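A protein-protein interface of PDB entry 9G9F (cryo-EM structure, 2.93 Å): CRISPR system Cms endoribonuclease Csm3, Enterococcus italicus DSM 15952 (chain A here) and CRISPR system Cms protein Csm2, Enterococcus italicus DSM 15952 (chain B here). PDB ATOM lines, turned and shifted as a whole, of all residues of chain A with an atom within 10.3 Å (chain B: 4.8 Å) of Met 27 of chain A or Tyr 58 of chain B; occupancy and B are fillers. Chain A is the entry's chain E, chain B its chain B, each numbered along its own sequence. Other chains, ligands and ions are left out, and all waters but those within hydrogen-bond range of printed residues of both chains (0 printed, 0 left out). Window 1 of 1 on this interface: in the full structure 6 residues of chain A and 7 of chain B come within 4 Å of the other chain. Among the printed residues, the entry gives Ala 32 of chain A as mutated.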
ATOM      1  N   GLY A  23      -6.698 -25.789  -3.097  1.00  0.00           N
ATOM      2  CA  GLY A  23      -7.614 -26.326  -4.081  1.00  0.00           C
ATOM      3  C   GLY A  23      -8.350 -25.296  -4.906  1.00  0.00           C
ATOM      4  O   GLY A  23      -9.137 -25.676  -5.781  1.00  0.00           O
ATOM      5  N   GLU A  24      -8.123 -24.010  -4.658  1.00  0.00           N
ATOM      6  CA  GLU A  24      -8.744 -22.932  -5.413  1.00  0.00           C
ATOM      7  C   GLU A  24      -7.657 -22.027  -5.968  1.00  0.00           C
ATOM      8  O   GLU A  24      -6.795 -21.556  -5.219  1.00  0.00           O
ATOM      9  CB  GLU A  24      -9.704 -22.126  -4.535  1.00  0.00           C
ATOM     10  CG  GLU A  24     -10.177 -20.827  -5.168  1.00  0.00           C
ATOM     11  CD  GLU A  24     -10.811 -19.888  -4.163  1.00  0.00           C
ATOM     12  OE1 GLU A  24     -10.876 -20.249  -2.969  1.00  0.00           O
ATOM     13  OE2 GLU A  24     -11.241 -18.788  -4.566  1.00  0.00           O
ATOM     14  N   THR A  25      -7.694 -21.793  -7.275  1.00  0.00           N
ATOM     15  CA  THR A  25      -6.744 -20.876  -7.884  1.00  0.00           C
ATOM     16  C   THR A  25      -7.102 -19.438  -7.528  1.00  0.00           C
ATOM     17  O   THR A  25      -8.275 -19.068  -7.432  1.00  0.00           O
ATOM     18  CB  THR A  25      -6.719 -21.052  -9.401  1.00  0.00           C
ATOM     19  OG1 THR A  25      -6.910 -22.434  -9.726  1.00  0.00           O
ATOM     20  CG2 THR A  25      -5.383 -20.594  -9.960  1.00  0.00           C
ATOM     21  N   SER A  26      -6.071 -18.625  -7.332  1.00  0.00           N
ATOM     22  CA  SER A  26      -6.257 -17.247  -6.897  1.00  0.00           C
ATOM     23  C   SER A  26      -6.625 -16.372  -8.088  1.00  0.00           C
ATOM     24  O   SER A  26      -5.856 -16.271  -9.048  1.00  0.00           O
ATOM     25  CB  SER A  26      -4.983 -16.733  -6.228  1.00  0.00           C
ATOM     26  OG  SER A  26      -4.981 -15.318  -6.140  1.00  0.00           O
ATOM     27  N   MET A  27      -7.798 -15.742  -8.032  1.00  0.00           N
ATOM     28  CA  MET A  27      -8.104 -14.707  -9.008  1.00  0.00           C
ATOM     29  C   MET A  27      -7.140 -13.547  -8.809  1.00  0.00           C
ATOM     30  O   MET A  27      -6.702 -13.273  -7.689  1.00  0.00           O
ATOM     31  CB  MET A  27      -9.556 -14.238  -8.878  1.00  0.00           C
ATOM     32  CG  MET A  27      -9.748 -12.743  -9.111  1.00  0.00           C
ATOM     33  SD  MET A  27     -11.457 -12.191  -9.178  1.00  0.00           S
ATOM     34  CE  MET A  27     -11.238 -10.517  -9.776  1.00  0.00           C
ATOM     35  N   ILE A  28      -6.693 -12.983  -9.938  1.00  0.00           N
ATOM     36  CA  ILE A  28      -5.648 -11.917  -9.875  1.00  0.00           C
ATOM     37  C   ILE A  28      -6.111 -10.789  -8.949  1.00  0.00           C
ATOM     38  O   ILE A  28      -7.208 -10.231  -9.173  1.00  0.00           O
ATOM     39  CB  ILE A  28      -5.250 -11.412 -11.276  1.00  0.00           C
ATOM     40  CG1 ILE A  28      -4.606 -12.526 -12.096  1.00  0.00           C
ATOM     41  CG2 ILE A  28      -4.330 -10.195 -11.183  1.00  0.00           C
ATOM     42  CD1 ILE A  28      -3.488 -13.256 -11.376  1.00  0.00           C
ATOM     43  N   GLY A  29      -5.291 -10.487  -7.948  1.00  0.00           N
ATOM     44  CA  GLY A  29      -5.593  -9.443  -6.995  1.00  0.00           C
ATOM     45  C   GLY A  29      -6.494  -9.858  -5.855  1.00  0.00           C
ATOM     46  O   GLY A  29      -6.804  -9.022  -4.999  1.00  0.00           O
ATOM     47  N   ALA A  30      -6.928 -11.112  -5.815  1.00  0.00           N
ATOM     48  CA  ALA A  30      -7.750 -11.618  -4.728  1.00  0.00           C
ATOM     49  C   ALA A  30      -6.847 -12.192  -3.639  1.00  0.00           C
ATOM     50  O   ALA A  30      -5.628 -11.997  -3.644  1.00  0.00           O
ATOM     51  CB  ALA A  30      -8.749 -12.646  -5.248  1.00  0.00           C
ATOM     52  N   ILE A  31      -7.443 -12.907  -2.685  1.00  0.00           N
ATOM     53  CA  ILE A  31      -6.691 -13.431  -1.552  1.00  0.00           C
ATOM     54  C   ILE A  31      -5.678 -14.460  -2.031  1.00  0.00           C
ATOM     55  O   ILE A  31      -6.011 -15.386  -2.784  1.00  0.00           O
ATOM     56  CB  ILE A  31      -7.648 -14.019  -0.505  1.00  0.00           C
ATOM     57  CG1 ILE A  31      -8.558 -15.070  -1.145  1.00  0.00           C
ATOM     58  CG2 ILE A  31      -8.457 -12.914   0.146  1.00  0.00           C
ATOM     59  CD1 ILE A  31      -9.810 -15.371  -0.358  1.00  0.00           C
ATOM     60  N   ALA A  32      -4.423 -14.286  -1.614  1.00  0.00           N
ATOM     61  CA  ALA A  32      -3.377 -15.226  -1.999  1.00  0.00           C
ATOM     62  C   ALA A  32      -3.485 -16.528  -1.217  1.00  0.00           C
ATOM     63  O   ALA A  32      -3.286 -17.613  -1.776  1.00  0.00           O
ATOM     64  CB  ALA A  32      -2.004 -14.591  -1.798  1.00  0.00           C
ATOM     65  N   SER A  33      -3.796 -16.443   0.077  1.00  0.00           N
ATOM     66  CA  SER A  33      -3.888 -17.606   0.959  1.00  0.00           C
ATOM     67  C   SER A  33      -5.262 -17.616   1.613  1.00  0.00           C
ATOM     68  O   SER A  33      -5.451 -17.036   2.692  1.00  0.00           O
ATOM     69  CB  SER A  33      -2.780 -17.586   2.009  1.00  0.00           C
ATOM     70  OG  SER A  33      -1.500 -17.645   1.403  1.00  0.00           O
ATOM     71  N   PRO A  34      -6.250 -18.255   0.996  1.00  0.00           N
ATOM     72  CA  PRO A  34      -7.588 -18.285   1.590  1.00  0.00           C
ATOM     73  C   PRO A  34      -7.626 -19.130   2.851  1.00  0.00           C
ATOM     74  O   PRO A  34      -6.864 -20.084   3.013  1.00  0.00           O
ATOM     75  CB  PRO A  34      -8.448 -18.905   0.486  1.00  0.00           C
ATOM     76  CG  PRO A  34      -7.499 -19.762  -0.270  1.00  0.00           C
ATOM     77  CD  PRO A  34      -6.174 -19.049  -0.240  1.00  0.00           C
ATOM     78  N   ARG A  37     -12.520 -23.206   4.575  1.00  0.00           N
ATOM     79  CA  ARG A  37     -13.947 -23.041   4.783  1.00  0.00           C
ATOM     80  C   ARG A  37     -14.634 -24.363   4.501  1.00  0.00           C
ATOM     81  O   ARG A  37     -14.242 -25.093   3.588  1.00  0.00           O
ATOM     82  CB  ARG A  37     -14.528 -21.954   3.871  1.00  0.00           C
ATOM     83  CG  ARG A  37     -13.862 -20.598   4.005  1.00  0.00           C
ATOM     84  CD  ARG A  37     -14.155 -19.715   2.809  1.00  0.00           C
ATOM     85  NE  ARG A  37     -13.957 -18.306   3.120  1.00  0.00           N
ATOM     86  CZ  ARG A  37     -14.941 -17.464   3.402  1.00  0.00           C
ATOM     87  NH1 ARG A  37     -16.204 -17.852   3.396  1.00  0.00           N
ATOM     88  NH2 ARG A  37     -14.652 -16.201   3.696  1.00  0.00           N
ATOM     89  N   ARG A  42     -19.859 -22.252   3.481  1.00  0.00           N
ATOM     90  CA  ARG A  42     -18.949 -21.182   3.076  1.00  0.00           C
ATOM     91  C   ARG A  42     -18.601 -20.276   4.252  1.00  0.00           C
ATOM     92  O   ARG A  42     -18.644 -19.050   4.147  1.00  0.00           O
ATOM     93  CB  ARG A  42     -19.524 -20.370   1.915  1.00  0.00           C
ATOM     94  CG  ARG A  42     -19.439 -21.070   0.570  1.00  0.00           C
ATOM     95  CD  ARG A  42     -19.773 -20.117  -0.569  1.00  0.00           C
ATOM     96  NE  ARG A  42     -18.866 -18.974  -0.644  1.00  0.00           N
ATOM     97  CZ  ARG A  42     -17.555 -19.045  -0.840  1.00  0.00           C
ATOM     98  NH1 ARG A  42     -16.942 -20.201  -1.043  1.00  0.00           N
ATOM     99  NH2 ARG A  42     -16.840 -17.924  -0.849  1.00  0.00           N
ATOM    100  N   THR A 121      -9.622  -9.542   4.981  1.00  0.00           N
ATOM    101  CA  THR A 121      -8.543  -9.691   4.010  1.00  0.00           C
ATOM    102  C   THR A 121      -7.401  -8.779   4.443  1.00  0.00           C
ATOM    103  O   THR A 121      -7.253  -7.640   3.992  1.00  0.00           O
ATOM    104  CB  THR A 121      -9.032  -9.371   2.603  1.00  0.00           C
ATOM    105  OG1 THR A 121     -10.051 -10.306   2.233  1.00  0.00           O
ATOM    106  CG2 THR A 121      -7.891  -9.483   1.604  1.00  0.00           C
ATOM    107  N   GLN A 138      -2.134 -11.015   0.408  1.00  0.00           N
ATOM    108  CA  GLN A 138      -3.445 -10.916   1.028  1.00  0.00           C
ATOM    109  C   GLN A 138      -3.710 -12.208   1.782  1.00  0.00           C
ATOM    110  O   GLN A 138      -3.682 -13.291   1.189  1.00  0.00           O
ATOM    111  CB  GLN A 138      -4.533 -10.654  -0.012  1.00  0.00           C
ATOM    112  CG  GLN A 138      -4.341  -9.363  -0.783  1.00  0.00           C
ATOM    113  CD  GLN A 138      -5.542  -9.015  -1.633  1.00  0.00           C
ATOM    114  OE1 GLN A 138      -6.637  -9.531  -1.422  1.00  0.00           O
ATOM    115  NE2 GLN A 138      -5.340  -8.144  -2.612  1.00  0.00           N
ATOM    116  N   GLU A 140      -6.441 -14.165   4.315  1.00  0.00           N
ATOM    117  CA  GLU A 140      -7.844 -14.127   4.714  1.00  0.00           C
ATOM    118  C   GLU A 140      -7.950 -14.599   6.161  1.00  0.00           C
ATOM    119  O   GLU A 140      -8.249 -15.758   6.452  1.00  0.00           O
ATOM    120  CB  GLU A 140      -8.681 -14.981   3.772  1.00  0.00           C
ATOM    121  CG  GLU A 140     -10.167 -14.724   3.830  1.00  0.00           C
ATOM    122  CD  GLU A 140     -10.953 -15.715   2.995  1.00  0.00           C
ATOM    123  OE1 GLU A 140     -10.371 -16.732   2.567  1.00  0.00           O
ATOM    124  OE2 GLU A 140     -12.151 -15.472   2.755  1.00  0.00           O
ATOM    125  N   LEU B  51      -8.681  -2.937 -10.971  1.00  0.00           N
ATOM    126  CA  LEU B  51      -8.818  -4.311 -10.509  1.00  0.00           C
ATOM    127  C   LEU B  51      -9.020  -4.382  -9.003  1.00  0.00           C
ATOM    128  O   LEU B  51      -9.650  -5.320  -8.513  1.00  0.00           O
ATOM    129  CB  LEU B  51      -7.594  -5.124 -10.919  1.00  0.00           C
ATOM    130  CG  LEU B  51      -7.723  -6.626 -10.694  1.00  0.00           C
ATOM    131  CD1 LEU B  51      -9.015  -7.155 -11.290  1.00  0.00           C
ATOM    132  CD2 LEU B  51      -6.533  -7.329 -11.288  1.00  0.00           C
ATOM    133  N   ILE B  54     -12.567  -3.888  -8.606  1.00  0.00           N
ATOM    134  CA  ILE B  54     -13.193  -5.134  -9.035  1.00  0.00           C
ATOM    135  C   ILE B  54     -13.119  -6.178  -7.928  1.00  0.00           C
ATOM    136  O   ILE B  54     -14.084  -6.899  -7.673  1.00  0.00           O
ATOM    137  CB  ILE B  54     -12.542  -5.641 -10.333  1.00  0.00           C
ATOM    138  CG1 ILE B  54     -12.782  -4.650 -11.465  1.00  0.00           C
ATOM    139  CG2 ILE B  54     -13.099  -6.997 -10.710  1.00  0.00           C
ATOM    140  CD1 ILE B  54     -14.220  -4.249 -11.608  1.00  0.00           C
ATOM    141  N   ASN B  55     -11.968  -6.280  -7.264  1.00  0.00           N
ATOM    142  CA  ASN B  55     -11.817  -7.225  -6.162  1.00  0.00           C
ATOM    143  C   ASN B  55     -12.733  -6.869  -5.003  1.00  0.00           C
ATOM    144  O   ASN B  55     -13.309  -7.756  -4.363  1.00  0.00           O
ATOM    145  CB  ASN B  55     -10.365  -7.258  -5.692  1.00  0.00           C
ATOM    146  CG  ASN B  55      -9.452  -7.936  -6.681  1.00  0.00           C
ATOM    147  OD1 ASN B  55      -9.791  -8.976  -7.242  1.00  0.00           O
ATOM    148  ND2 ASN B  55      -8.282  -7.351  -6.904  1.00  0.00           N
ATOM    149  N   HIS B  56     -12.864  -5.575  -4.708  1.00  0.00           N
ATOM    150  CA  HIS B  56     -13.704  -5.162  -3.591  1.00  0.00           C
ATOM    151  C   HIS B  56     -15.159  -5.549  -3.822  1.00  0.00           C
ATOM    152  O   HIS B  56     -15.837  -6.011  -2.898  1.00  0.00           O
ATOM    153  CB  HIS B  56     -13.570  -3.659  -3.355  1.00  0.00           C
ATOM    154  CG  HIS B  56     -14.165  -3.200  -2.061  1.00  0.00           C
ATOM    155  ND1 HIS B  56     -14.332  -1.869  -1.747  1.00  0.00           N
ATOM    156  CD2 HIS B  56     -14.644  -3.899  -1.004  1.00  0.00           C
ATOM    157  CE1 HIS B  56     -14.884  -1.766  -0.551  1.00  0.00           C
ATOM    158  NE2 HIS B  56     -15.084  -2.983  -0.079  1.00  0.00           N
ATOM    159  N   VAL B  57     -15.662  -5.363  -5.043  1.00  0.00           N
ATOM    160  CA  VAL B  57     -17.029  -5.824  -5.299  1.00  0.00           C
ATOM    161  C   VAL B  57     -17.094  -7.354  -5.394  1.00  0.00           C
ATOM    162  O   VAL B  57     -18.067  -7.974  -4.933  1.00  0.00           O
ATOM    163  CB  VAL B  57     -17.612  -5.147  -6.554  1.00  0.00           C
ATOM    164  CG1 VAL B  57     -16.684  -5.288  -7.737  1.00  0.00           C
ATOM    165  CG2 VAL B  57     -18.982  -5.719  -6.880  1.00  0.00           C
ATOM    166  N   TYR B  58     -16.064  -7.985  -5.962  1.00  0.00           N
ATOM    167  CA  TYR B  58     -16.092  -9.417  -6.226  1.00  0.00           C
ATOM    168  C   TYR B  58     -16.054 -10.235  -4.947  1.00  0.00           C
ATOM    169  O   TYR B  58     -16.638 -11.318  -4.899  1.00  0.00           O
ATOM    170  CB  TYR B  58     -14.916  -9.787  -7.128  1.00  0.00           C
ATOM    171  CG  TYR B  58     -14.528 -11.247  -7.115  1.00  0.00           C
ATOM    172  CD1 TYR B  58     -15.259 -12.188  -7.825  1.00  0.00           C
ATOM    173  CD2 TYR B  58     -13.426 -11.683  -6.394  1.00  0.00           C
ATOM    174  CE1 TYR B  58     -14.902 -13.520  -7.822  1.00  0.00           C
ATOM    175  CE2 TYR B  58     -13.066 -13.013  -6.379  1.00  0.00           C
ATOM    176  CZ  TYR B  58     -13.804 -13.926  -7.096  1.00  0.00           C
ATOM    177  OH  TYR B  58     -13.436 -15.251  -7.085  1.00  0.00           O
ATOM    178  N   THR B  59     -15.359  -9.756  -3.915  1.00  0.00           N
ATOM    179  CA  THR B  59     -15.337 -10.483  -2.649  1.00  0.00           C
ATOM    180  C   THR B  59     -16.734 -10.565  -2.049  1.00  0.00           C
ATOM    181  O   THR B  59     -17.181 -11.636  -1.616  1.00  0.00           O
ATOM    182  CB  THR B  59     -14.373  -9.811  -1.674  1.00  0.00           C
ATOM    183  OG1 THR B  59     -13.057  -9.794  -2.239  1.00  0.00           O
ATOM    184  CG2 THR B  59     -14.340 -10.572  -0.364  1.00  0.00           C
ATOM    185  N   LYS B  60     -17.451  -9.441  -2.041  1.00  0.00           N
ATOM    186  CA  LYS B  60     -18.822  -9.438  -1.546  1.00  0.00           C
ATOM    187  C   LYS B  60     -19.714 -10.320  -2.405  1.00  0.00           C
ATOM    188  O   LYS B  60     -20.593 -11.018  -1.885  1.00  0.00           O
ATOM    189  CB  LYS B  60     -19.362  -8.010  -1.504  1.00  0.00           C
ATOM    190  CG  LYS B  60     -18.534  -7.062  -0.658  1.00  0.00           C
ATOM    191  CD  LYS B  60     -19.383  -5.929  -0.115  1.00  0.00           C
ATOM    192  CE  LYS B  60     -20.216  -5.294  -1.215  1.00  0.00           C
ATOM    193  NZ  LYS B  60     -20.994  -4.136  -0.706  1.00  0.00           N
ATOM    194  N   VAL B  61     -19.515 -10.296  -3.724  1.00  0.00           N
ATOM    195  CA  VAL B  61     -20.331 -11.142  -4.592  1.00  0.00           C
ATOM    196  C   VAL B  61     -20.067 -12.618  -4.314  1.00  0.00           C
ATOM    197  O   VAL B  61     -21.001 -13.427  -4.244  1.00  0.00           O
ATOM    198  CB  VAL B  61     -20.086 -10.793  -6.068  1.00  0.00           C
ATOM    199  CG1 VAL B  61     -20.748 -11.822  -6.963  1.00  0.00           C
ATOM    200  CG2 VAL B  61     -20.611  -9.402  -6.372  1.00  0.00           C
ATOM    201  N   TYR B  62     -18.792 -12.966  -4.126  1.00  0.00           N
ATOM    202  CA  TYR B  62     -18.415 -14.391  -3.916  1.00  0.00           C
ATOM    203  C   TYR B  62     -18.933 -14.892  -2.571  1.00  0.00           C
ATOM    204  O   TYR B  62     -19.391 -16.053  -2.499  1.00  0.00           O
ATOM    205  CB  TYR B  62     -16.888 -14.455  -4.014  1.00  0.00           C
ATOM    206  CG  TYR B  62     -16.270 -15.846  -3.950  1.00  0.00           C
ATOM    207  CD1 TYR B  62     -16.939 -16.958  -4.446  1.00  0.00           C
ATOM    208  CD2 TYR B  62     -15.010 -16.040  -3.399  1.00  0.00           C
ATOM    209  CE1 TYR B  62     -16.377 -18.222  -4.388  1.00  0.00           C
ATOM    210  CE2 TYR B  62     -14.435 -17.298  -3.338  1.00  0.00           C
ATOM    211  CZ  TYR B  62     -15.121 -18.393  -3.834  1.00  0.00           C
ATOM    212  OH  TYR B  62     -14.558 -19.634  -3.774  1.00  0.00           O
ATOM    213  N   PHE B 119     -21.709 -11.428 -13.706  1.00  0.00           N
ATOM    214  CA  PHE B 119     -20.677 -10.698 -12.979  1.00  0.00           C
ATOM    215  C   PHE B 119     -19.395 -11.510 -12.887  1.00  0.00           C
ATOM    216  O   PHE B 119     -18.292 -10.960 -12.984  1.00  0.00           O
ATOM    217  CB  PHE B 119     -21.174 -10.332 -11.583  1.00  0.00           C
ATOM    218  CG  PHE B 119     -20.126  -9.702 -10.714  1.00  0.00           C
ATOM    219  CD1 PHE B 119     -19.883  -8.345 -10.773  1.00  0.00           C
ATOM    220  CD2 PHE B 119     -19.378 -10.470  -9.842  1.00  0.00           C
ATOM    221  CE1 PHE B 119     -18.921  -7.767  -9.978  1.00  0.00           C
ATOM    222  CE2 PHE B 119     -18.412  -9.898  -9.048  1.00  0.00           C
ATOM    223  CZ  PHE B 119     -18.186  -8.545  -9.114  1.00  0.00           C
ATOM    224  N   LEU B 120     -19.518 -12.823 -12.678  1.00  0.00           N
ATOM    225  CA  LEU B 120     -18.327 -13.655 -12.547  1.00  0.00           C
ATOM    226  C   LEU B 120     -17.536 -13.716 -13.851  1.00  0.00           C
ATOM    227  O   LEU B 120     -16.306 -13.595 -13.838  1.00  0.00           O
ATOM    228  CB  LEU B 120     -18.714 -15.054 -12.077  1.00  0.00           C
ATOM    229  CG  LEU B 120     -18.464 -15.280 -10.586  1.00  0.00           C
ATOM    230  CD1 LEU B 120     -16.975 -15.247 -10.294  1.00  0.00           C
ATOM    231  CD2 LEU B 120     -19.189 -14.243  -9.751  1.00  0.00           C
ATOM    232  N   CYS B 123     -15.734 -10.458 -14.231  1.00  0.00           N
ATOM    233  CA  CYS B 123     -14.509 -10.426 -13.439  1.00  0.00           C
ATOM    234  C   CYS B 123     -13.414 -11.266 -14.082  1.00  0.00           C
ATOM    235  O   CYS B 123     -12.239 -10.880 -14.070  1.00  0.00           O
ATOM    236  CB  CYS B 123     -14.790 -10.906 -12.017  1.00  0.00           C
ATOM    237  SG  CYS B 123     -15.513  -9.648 -10.949  1.00  0.00           S
ATOM    238  N   GLU B 127      -9.781  -9.858 -15.230  1.00  0.00           N
ATOM    239  CA  GLU B 127      -8.539 -10.477 -14.787  1.00  0.00           C
ATOM    240  C   GLU B 127      -7.706 -10.946 -15.974  1.00  0.00           C
ATOM    241  O   GLU B 127      -6.474 -10.853 -15.953  1.00  0.00           O
ATOM    242  CB  GLU B 127      -8.852 -11.629 -13.836  1.00  0.00           C
ATOM    243  CG  GLU B 127      -7.700 -12.562 -13.582  1.00  0.00           C
ATOM    244  CD  GLU B 127      -8.146 -13.901 -13.043  1.00  0.00           C
ATOM    245  OE1 GLU B 127      -7.276 -14.762 -12.817  1.00  0.00           O
ATOM    246  OE2 GLU B 127      -9.363 -14.092 -12.840  1.00  0.00           O
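The side-chain amide nitrogen (ND2) of Asn 55 of chain B is in hydrogen-bond range of the backbone carbonyl oxygen (O) of Leu 51 of chain B, 2.9 Å away.
The backbone carbonyl oxygen (O) of Asn 55 of chain B lies within hydrogen-bond range of the side-chain hydroxyl (OG1) of Thr 59 of chain B (3.0 Å).
O of Gly 29 of chain A sits at hydrogen-bond distance from NE2 of Gln 138 of chain A.
The side-chain amide oxygen of Gln 138 of chain A sits close to the backbone carbonyl oxygen of Ala 30 of chain A.
NH1 of Arg 37 of chain A lies within hydrogen-bond range of O of Arg 42 of chain A (2.8 Å).
Hydrophobic or aromatic side chains of chain A that line the printed part of chain B: Met 27 and Ile 28.
Of the 14 printed residues of chain B, 5 touch a printed residue of chain A.
Hydrophobic or aromatic side chains of chain B that line the printed part of chain A: Leu 51, Tyr 58 and Tyr 62.
Along chain B the printed residues that touch a printed residue of chain A span positions 51 to 127.
Among the printed residues, 10 pairs touch across the chains.
The side-chain amide oxygen (OD1) of Asn 55 of chain B lies close to the backbone carbonyl oxygen (O) of Ile 28 of chain A.
The backbone carbonyl oxygen of Gly 29 of chain A is in hydrogen-bond range of the side-chain amide nitrogen of Asn 55 of chain B (2.9 Å).
NE of Arg 42 of chain A sits at hydrogen-bond distance from O of Tyr 62 of chain B (3.5 Å).
OE1 of Glu 127 of chain B sits at hydrogen-bond distance from N of Ile 28 of chain A (3.4 Å).
Printed residues of chain B within 4 Å of Met 27 of chain A: Asn 55, Tyr 58 and Glu 127.
Asn 55 of chain B touches just these residues of chain A: Met 27 (3.3 Å), Ile 28 (3.5 Å), Gly 29 (2.9 Å) and Ala 30 (3.8 Å).
No residue of chain A comes within 4 Å of Val 57 of chain B.
No residue of chain A comes within 4 Å of Thr 59 of chain B.
No residue of chain A comes within 4 Å of Val 61 of chain B.
Of chain A, only Glu 24 (3.5 Å) and Arg 42 (3.5 Å) come within 4 Å of Tyr 62 of chain B.
Of the printed residues of chain B, Glu 24 of chain A touches Tyr 62.
Printed residues of chain B within 4 Å of Ala 30 of chain A: Asn 55 (3.8 Å).
Ile 54 of chain B touches none of the printed residues of chain A.
Arg 37 of chain A touches none of the printed residues of chain B.
The nearest residue of chain B that does not touch Met 27 of chain A is Ile 54 of chain B (4.1 Å).
The nearest residue of chain A that does not touch Tyr 58 of chain B is Ala 30 of chain A (4.5 Å).
Glu 24 of chain A touches Tyr 62 of chain B.
Met 27 of chain A touches Asn 55 of chain B.
Tyr 58 of chain B touches Met 27 of chain A.
Met 27 of chain A touches Glu 127 of chain B.
CG2 of Ile 28 of chain A touches CD2 of Leu 51 of chain B, 3.6 Å away.
Asn 55 of chain B touches Ala 30 of chain A.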
